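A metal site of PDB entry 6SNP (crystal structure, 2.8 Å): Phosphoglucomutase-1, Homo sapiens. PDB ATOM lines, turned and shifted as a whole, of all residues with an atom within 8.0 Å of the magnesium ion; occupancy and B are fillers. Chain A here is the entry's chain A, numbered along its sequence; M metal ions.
The magnesium ion is bound by the side-chain hydroxyl of Ser 138, the side-chain carboxylate of Asp 313, the side-chain carboxylate of Asp 309 and the side-chain carboxylate of Asp 311.
The magnesium ion has four donor atoms within binding distance.
The backbone NH (N) of Gly 310 sits close to the backbone carbonyl oxygen (O) of Ser 138 (3.5 Å).
OG of Ser 138 lies close to ND1 of His 139, 3.4 Å away.
The backbone carbonyl oxygen (O) of Ser 399 lies close to the guanidinium group (NE) of Arg 314 (3.2 Å).
The side-chain hydroxyl of Thr 117 sits at hydrogen-bond distance from the side-chain carboxylate of Asp 311 (2.7 Å).
The side-chain carboxylate of Asp 309 lies within hydrogen-bond range of the backbone NH of Gly 312 (3.0 Å).
The guanidinium group (NH1) of Arg 314 is in salt-bridge range of the side-chain carboxylate (OD1) of Asp 284 (3.4 Å).
The backbone NH (N) of Ser 138 lies within hydrogen-bond range of the side-chain hydroxyl (OG1) of Thr 136 (2.8 Å).
The side-chain carboxylate of Asp 309 sits at hydrogen-bond distance from the backbone NH of Arg 314 (3.0 Å).
Merely in contact with the magnesium ion: Arg 314 (3.6 Å).
Of the 26 residues printed, 5 come within 4 Å of the magnesium ion.
The nearest printed residue that does not touch the magnesium ion is His 139 (4.5 Å).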
ATOM      1  N   SER A  41      15.263 -20.268   3.290  1.00  0.00           N
ATOM      2  CA  SER A  41      16.617 -20.690   3.616  1.00  0.00           C
ATOM      3  C   SER A  41      17.632 -20.207   2.586  1.00  0.00           C
ATOM      4  O   SER A  41      18.649 -20.879   2.341  1.00  0.00           O
ATOM      5  CB  SER A  41      16.668 -22.210   3.746  1.00  0.00           C
ATOM      6  OG  SER A  41      16.050 -22.645   4.944  1.00  0.00           O
ATOM      7  N   ARG A  44      19.755 -22.008  -2.813  1.00  0.00           N
ATOM      8  CA  ARG A  44      20.635 -23.160  -2.959  1.00  0.00           C
ATOM      9  C   ARG A  44      20.470 -23.754  -4.352  1.00  0.00           C
ATOM     10  O   ARG A  44      19.344 -24.106  -4.746  1.00  0.00           O
ATOM     11  CB  ARG A  44      20.361 -24.234  -1.904  1.00  0.00           C
ATOM     12  CG  ARG A  44      19.961 -23.715  -0.540  1.00  0.00           C
ATOM     13  CD  ARG A  44      20.281 -24.769   0.510  1.00  0.00           C
ATOM     14  NE  ARG A  44      19.753 -24.455   1.836  1.00  0.00           N
ATOM     15  CZ  ARG A  44      20.221 -23.501   2.637  1.00  0.00           C
ATOM     16  NH1 ARG A  44      21.232 -22.728   2.245  1.00  0.00           N
ATOM     17  NH2 ARG A  44      19.676 -23.310   3.827  1.00  0.00           N
ATOM     18  N   ASP A  83      30.102 -21.699   5.977  1.00  0.00           N
ATOM     19  CA  ASP A  83      30.318 -22.917   6.747  1.00  0.00           C
ATOM     20  C   ASP A  83      31.596 -23.648   6.360  1.00  0.00           C
ATOM     21  O   ASP A  83      31.963 -24.602   7.035  1.00  0.00           O
ATOM     22  CB  ASP A  83      29.132 -23.860   6.585  1.00  0.00           C
ATOM     23  CG  ASP A  83      28.681 -23.996   5.122  1.00  0.00           C
ATOM     24  OD1 ASP A  83      29.333 -23.394   4.231  1.00  0.00           O
ATOM     25  OD2 ASP A  83      27.665 -24.697   4.874  1.00  0.00           O
ATOM     26  N   THR A 117      26.144 -19.879  11.113  1.00  0.00           N
ATOM     27  CA  THR A 117      24.946 -19.048  11.038  1.00  0.00           C
ATOM     28  C   THR A 117      24.591 -18.397  12.373  1.00  0.00           C
ATOM     29  O   THR A 117      24.341 -17.177  12.398  1.00  0.00           O
ATOM     30  CB  THR A 117      23.773 -19.891  10.504  1.00  0.00           C
ATOM     31  OG1 THR A 117      24.089 -20.352   9.185  1.00  0.00           O
ATOM     32  CG2 THR A 117      22.507 -19.059  10.446  1.00  0.00           C
ATOM     33  N   PRO A 118      24.579 -19.110  13.515  1.00  0.00           N
ATOM     34  CA  PRO A 118      24.383 -18.403  14.789  1.00  0.00           C
ATOM     35  C   PRO A 118      25.449 -17.364  15.063  1.00  0.00           C
ATOM     36  O   PRO A 118      25.144 -16.294  15.616  1.00  0.00           O
ATOM     37  CB  PRO A 118      24.421 -19.538  15.828  1.00  0.00           C
ATOM     38  CG  PRO A 118      24.054 -20.765  15.061  1.00  0.00           C
ATOM     39  CD  PRO A 118      24.674 -20.571  13.715  1.00  0.00           C
ATOM     40  N   THR A 136      26.267 -20.916   2.787  1.00  0.00           N
ATOM     41  CA  THR A 136      25.998 -22.255   3.293  1.00  0.00           C
ATOM     42  C   THR A 136      24.798 -22.844   2.556  1.00  0.00           C
ATOM     43  O   THR A 136      23.910 -22.119   2.109  1.00  0.00           O
ATOM     44  CB  THR A 136      25.739 -22.261   4.802  1.00  0.00           C
ATOM     45  OG1 THR A 136      25.397 -23.585   5.227  1.00  0.00           O
ATOM     46  CG2 THR A 136      24.600 -21.308   5.152  1.00  0.00           C
ATOM     47  N   ALA A 137      24.802 -24.178   2.431  1.00  0.00           N
ATOM     48  CA  ALA A 137      23.617 -24.929   2.042  1.00  0.00           C
ATOM     49  C   ALA A 137      23.088 -25.748   3.211  1.00  0.00           C
ATOM     50  O   ALA A 137      22.379 -26.743   2.993  1.00  0.00           O
ATOM     51  CB  ALA A 137      23.906 -25.824   0.836  1.00  0.00           C
ATOM     52  N   SER A 138      23.440 -25.363   4.436  1.00  0.00           N
ATOM     53  CA  SER A 138      22.967 -25.997   5.673  1.00  0.00           C
ATOM     54  C   SER A 138      23.335 -27.469   5.652  1.00  0.00           C
ATOM     55  O   SER A 138      24.530 -27.788   5.581  1.00  0.00           O
ATOM     56  CB  SER A 138      21.471 -25.691   5.840  1.00  0.00           C
ATOM     57  OG  SER A 138      21.008 -26.125   7.101  1.00  0.00           O
ATOM     58  N   HIS A 139      22.367 -28.393   5.687  1.00  0.00           N
ATOM     59  CA  HIS A 139      22.628 -29.811   5.810  1.00  0.00           C
ATOM     60  C   HIS A 139      22.930 -30.493   4.479  1.00  0.00           C
ATOM     61  O   HIS A 139      23.245 -31.692   4.475  1.00  0.00           O
ATOM     62  CB  HIS A 139      21.427 -30.494   6.467  1.00  0.00           C
ATOM     63  CG  HIS A 139      20.116 -30.157   5.822  1.00  0.00           C
ATOM     64  ND1 HIS A 139      19.457 -28.960   6.057  1.00  0.00           N
ATOM     65  CD2 HIS A 139      19.345 -30.841   4.945  1.00  0.00           C
ATOM     66  CE1 HIS A 139      18.343 -28.941   5.351  1.00  0.00           C
ATOM     67  NE2 HIS A 139      18.251 -30.068   4.674  1.00  0.00           N
ATOM     68  N   ASN A 140      22.841 -29.779   3.359  1.00  0.00           N
ATOM     69  CA  ASN A 140      23.083 -30.385   2.063  1.00  0.00           C
ATOM     70  C   ASN A 140      24.569 -30.717   1.900  1.00  0.00           C
ATOM     71  O   ASN A 140      25.418 -30.130   2.563  1.00  0.00           O
ATOM     72  CB  ASN A 140      22.631 -29.436   0.944  1.00  0.00           C
ATOM     73  CG  ASN A 140      21.119 -29.268   0.916  1.00  0.00           C
ATOM     74  OD1 ASN A 140      20.382 -30.186   1.281  1.00  0.00           O
ATOM     75  ND2 ASN A 140      20.667 -28.105   0.473  1.00  0.00           N
ATOM     76  N   LYS A 151      22.615 -17.212   1.775  1.00  0.00           N
ATOM     77  CA  LYS A 151      21.592 -16.620   2.608  1.00  0.00           C
ATOM     78  C   LYS A 151      21.923 -15.161   2.872  1.00  0.00           C
ATOM     79  O   LYS A 151      23.098 -14.765   2.882  1.00  0.00           O
ATOM     80  CB  LYS A 151      21.470 -17.364   3.951  1.00  0.00           C
ATOM     81  CG  LYS A 151      21.150 -18.835   3.827  1.00  0.00           C
ATOM     82  CD  LYS A 151      20.949 -19.480   5.196  1.00  0.00           C
ATOM     83  CE  LYS A 151      19.780 -18.850   5.938  1.00  0.00           C
ATOM     84  NZ  LYS A 151      19.520 -19.540   7.231  1.00  0.00           N
ATOM     85  N   PRO A 283      26.204 -33.401   5.804  1.00  0.00           N
ATOM     86  CA  PRO A 283      26.252 -32.829   7.167  1.00  0.00           C
ATOM     87  C   PRO A 283      24.861 -32.608   7.748  1.00  0.00           C
ATOM     88  O   PRO A 283      24.438 -31.487   8.016  1.00  0.00           O
ATOM     89  CB  PRO A 283      27.013 -31.519   6.937  1.00  0.00           C
ATOM     90  CG  PRO A 283      26.629 -31.117   5.557  1.00  0.00           C
ATOM     91  CD  PRO A 283      26.485 -32.397   4.765  1.00  0.00           C
ATOM     92  N   ASP A 284      24.136 -33.706   7.932  1.00  0.00           N
ATOM     93  CA  ASP A 284      22.758 -33.671   8.428  1.00  0.00           C
ATOM     94  C   ASP A 284      22.669 -34.500   9.701  1.00  0.00           C
ATOM     95  O   ASP A 284      22.910 -35.718   9.654  1.00  0.00           O
ATOM     96  CB  ASP A 284      21.787 -34.195   7.372  1.00  0.00           C
ATOM     97  CG  ASP A 284      20.344 -33.879   7.694  1.00  0.00           C
ATOM     98  OD1 ASP A 284      20.093 -33.135   8.668  1.00  0.00           O
ATOM     99  OD2 ASP A 284      19.453 -34.377   6.972  1.00  0.00           O
ATOM    100  N   PRO A 285      22.351 -33.902  10.837  1.00  0.00           N
ATOM    101  CA  PRO A 285      22.289 -34.683  12.085  1.00  0.00           C
ATOM    102  C   PRO A 285      20.940 -35.351  12.292  1.00  0.00           C
ATOM    103  O   PRO A 285      19.994 -34.743  12.804  1.00  0.00           O
ATOM    104  CB  PRO A 285      22.573 -33.633  13.162  1.00  0.00           C
ATOM    105  CG  PRO A 285      22.058 -32.357  12.577  1.00  0.00           C
ATOM    106  CD  PRO A 285      22.178 -32.459  11.072  1.00  0.00           C
ATOM    107  N   PHE A 308      25.924 -31.879  14.884  1.00  0.00           N
ATOM    108  CA  PHE A 308      25.588 -30.601  14.253  1.00  0.00           C
ATOM    109  C   PHE A 308      25.509 -30.772  12.741  1.00  0.00           C
ATOM    110  O   PHE A 308      25.950 -31.772  12.170  1.00  0.00           O
ATOM    111  CB  PHE A 308      26.607 -29.525  14.604  1.00  0.00           C
ATOM    112  CG  PHE A 308      26.819 -29.345  16.080  1.00  0.00           C
ATOM    113  CD1 PHE A 308      25.781 -28.943  16.896  1.00  0.00           C
ATOM    114  CD2 PHE A 308      28.069 -29.565  16.636  1.00  0.00           C
ATOM    115  CE1 PHE A 308      25.979 -28.771  18.246  1.00  0.00           C
ATOM    116  CE2 PHE A 308      28.276 -29.389  17.988  1.00  0.00           C
ATOM    117  CZ  PHE A 308      27.220 -28.994  18.801  1.00  0.00           C
ATOM    118  N   ASP A 309      24.958 -29.752  12.086  1.00  0.00           N
ATOM    119  CA  ASP A 309      24.843 -29.760  10.647  1.00  0.00           C
ATOM    120  C   ASP A 309      25.907 -28.842  10.029  1.00  0.00           C
ATOM    121  O   ASP A 309      26.870 -28.444  10.692  1.00  0.00           O
ATOM    122  CB  ASP A 309      23.414 -29.345  10.244  1.00  0.00           C
ATOM    123  CG  ASP A 309      23.157 -27.871  10.434  1.00  0.00           C
ATOM    124  OD1 ASP A 309      23.613 -27.313  11.458  1.00  0.00           O
ATOM    125  OD2 ASP A 309      22.486 -27.279   9.570  1.00  0.00           O
ATOM    126  N   GLY A 310      25.739 -28.515   8.751  1.00  0.00           N
ATOM    127  CA  GLY A 310      26.693 -27.717   8.019  1.00  0.00           C
ATOM    128  C   GLY A 310      26.969 -26.359   8.625  1.00  0.00           C
ATOM    129  O   GLY A 310      28.112 -26.054   8.949  1.00  0.00           O
ATOM    130  N   ASP A 311      25.926 -25.553   8.796  1.00  0.00           N
ATOM    131  CA  ASP A 311      26.069 -24.170   9.245  1.00  0.00           C
ATOM    132  C   ASP A 311      25.815 -23.980  10.736  1.00  0.00           C
ATOM    133  O   ASP A 311      25.908 -22.849  11.225  1.00  0.00           O
ATOM    134  CB  ASP A 311      25.152 -23.247   8.440  1.00  0.00           C
ATOM    135  CG  ASP A 311      23.688 -23.564   8.634  1.00  0.00           C
ATOM    136  OD1 ASP A 311      23.374 -24.736   8.930  1.00  0.00           O
ATOM    137  OD2 ASP A 311      22.847 -22.656   8.494  1.00  0.00           O
ATOM    138  N   GLY A 312      25.501 -25.042  11.458  1.00  0.00           N
ATOM    139  CA  GLY A 312      25.498 -24.996  12.916  1.00  0.00           C
ATOM    140  C   GLY A 312      24.208 -24.547  13.576  1.00  0.00           C
ATOM    141  O   GLY A 312      24.257 -24.070  14.719  1.00  0.00           O
ATOM    142  N   ASP A 313      23.061 -24.693  12.918  1.00  0.00           N
ATOM    143  CA  ASP A 313      21.776 -24.370  13.521  1.00  0.00           C
ATOM    144  C   ASP A 313      20.978 -25.608  13.895  1.00  0.00           C
ATOM    145  O   ASP A 313      19.907 -25.478  14.499  1.00  0.00           O
ATOM    146  CB  ASP A 313      20.956 -23.481  12.576  1.00  0.00           C
ATOM    147  CG  ASP A 313      20.960 -23.974  11.145  1.00  0.00           C
ATOM    148  OD1 ASP A 313      21.373 -25.133  10.914  1.00  0.00           O
ATOM    149  OD2 ASP A 313      20.558 -23.208  10.251  1.00  0.00           O
ATOM    150  N   ARG A 314      21.464 -26.804  13.551  1.00  0.00           N
ATOM    151  CA  ARG A 314      20.818 -28.058  13.898  1.00  0.00           C
ATOM    152  C   ARG A 314      21.609 -28.769  14.998  1.00  0.00           C
ATOM    153  O   ARG A 314      22.797 -28.512  15.206  1.00  0.00           O
ATOM    154  CB  ARG A 314      20.704 -28.980  12.685  1.00  0.00           C
ATOM    155  CG  ARG A 314      20.094 -28.323  11.456  1.00  0.00           C
ATOM    156  CD  ARG A 314      18.594 -28.289  11.531  1.00  0.00           C
ATOM    157  NE  ARG A 314      17.972 -28.218  10.210  1.00  0.00           N
ATOM    158  CZ  ARG A 314      17.815 -29.262   9.409  1.00  0.00           C
ATOM    159  NH1 ARG A 314      18.237 -30.460   9.770  1.00  0.00           N
ATOM    160  NH2 ARG A 314      17.233 -29.093   8.222  1.00  0.00           N
ATOM    161  N   ASN A 315      20.926 -29.675  15.684  1.00  0.00           N
ATOM    162  CA  ASN A 315      21.562 -30.447  16.743  1.00  0.00           C
ATOM    163  C   ASN A 315      20.777 -31.725  16.962  1.00  0.00           C
ATOM    164  O   ASN A 315      19.542 -31.731  16.882  1.00  0.00           O
ATOM    165  CB  ASN A 315      21.660 -29.641  18.038  1.00  0.00           C
ATOM    166  CG  ASN A 315      20.313 -29.446  18.706  1.00  0.00           C
ATOM    167  OD1 ASN A 315      19.934 -30.222  19.585  1.00  0.00           O
ATOM    168  ND2 ASN A 315      19.580 -28.422  18.273  1.00  0.00           N
ATOM    169  N   SER A 399      12.681 -30.624  12.899  1.00  0.00           N
ATOM    170  CA  SER A 399      13.811 -30.729  11.991  1.00  0.00           C
ATOM    171  C   SER A 399      15.113 -30.454  12.729  1.00  0.00           C
ATOM    172  O   SER A 399      16.025 -29.818  12.187  1.00  0.00           O
ATOM    173  CB  SER A 399      13.638 -29.751  10.820  1.00  0.00           C
ATOM    174  OG  SER A 399      13.488 -28.432  11.293  1.00  0.00           O
ATOM    175  N   PHE A 400      15.211 -30.941  13.972  1.00  0.00           N
ATOM    176  CA  PHE A 400      16.402 -30.770  14.812  1.00  0.00           C
ATOM    177  C   PHE A 400      16.708 -29.290  15.025  1.00  0.00           C
ATOM    178  O   PHE A 400      17.863 -28.859  14.992  1.00  0.00           O
ATOM    179  CB  PHE A 400      17.608 -31.501  14.212  1.00  0.00           C
ATOM    180  CG  PHE A 400      17.400 -32.982  14.093  1.00  0.00           C
ATOM    181  CD1 PHE A 400      17.788 -33.829  15.115  1.00  0.00           C
ATOM    182  CD2 PHE A 400      16.811 -33.532  12.966  1.00  0.00           C
ATOM    183  CE1 PHE A 400      17.605 -35.194  15.019  1.00  0.00           C
ATOM    184  CE2 PHE A 400      16.617 -34.894  12.856  1.00  0.00           C
ATOM    185  CZ  PHE A 400      17.009 -35.726  13.887  1.00  0.00           C
ATOM    186  N   GLU A 409      18.496 -16.629  14.792  1.00  0.00           N
ATOM    187  CA  GLU A 409      18.670 -17.884  14.082  1.00  0.00           C
ATOM    188  C   GLU A 409      18.719 -18.993  15.118  1.00  0.00           C
ATOM    189  O   GLU A 409      19.020 -18.754  16.288  1.00  0.00           O
ATOM    190  CB  GLU A 409      19.953 -17.902  13.229  1.00  0.00           C
ATOM    191  CG  GLU A 409      19.910 -17.029  11.982  1.00  0.00           C
ATOM    192  CD  GLU A 409      19.391 -17.767  10.762  1.00  0.00           C
ATOM    193  OE1 GLU A 409      18.808 -18.860  10.923  1.00  0.00           O
ATOM    194  OE2 GLU A 409      19.561 -17.252   9.642  1.00  0.00           O
ATOM    195  N   LYS A 410      18.416 -20.211  14.686  1.00  0.00           N
ATOM    196  CA  LYS A 410      18.515 -21.348  15.592  1.00  0.00           C
ATOM    197  C   LYS A 410      19.975 -21.722  15.785  1.00  0.00           C
ATOM    198  O   LYS A 410      20.837 -21.446  14.942  1.00  0.00           O
ATOM    199  CB  LYS A 410      17.704 -22.525  15.066  1.00  0.00           C
ATOM    200  CG  LYS A 410      16.262 -22.465  15.544  1.00  0.00           C
ATOM    201  CD  LYS A 410      15.379 -23.475  14.844  1.00  0.00           C
ATOM    202  CE  LYS A 410      14.000 -23.478  15.483  1.00  0.00           C
ATOM    203  NZ  LYS A 410      13.416 -22.112  15.584  1.00  0.00           N
HETATM  204 MG    MG M   1      21.052 -25.766   9.048  1.00  0.00          MG
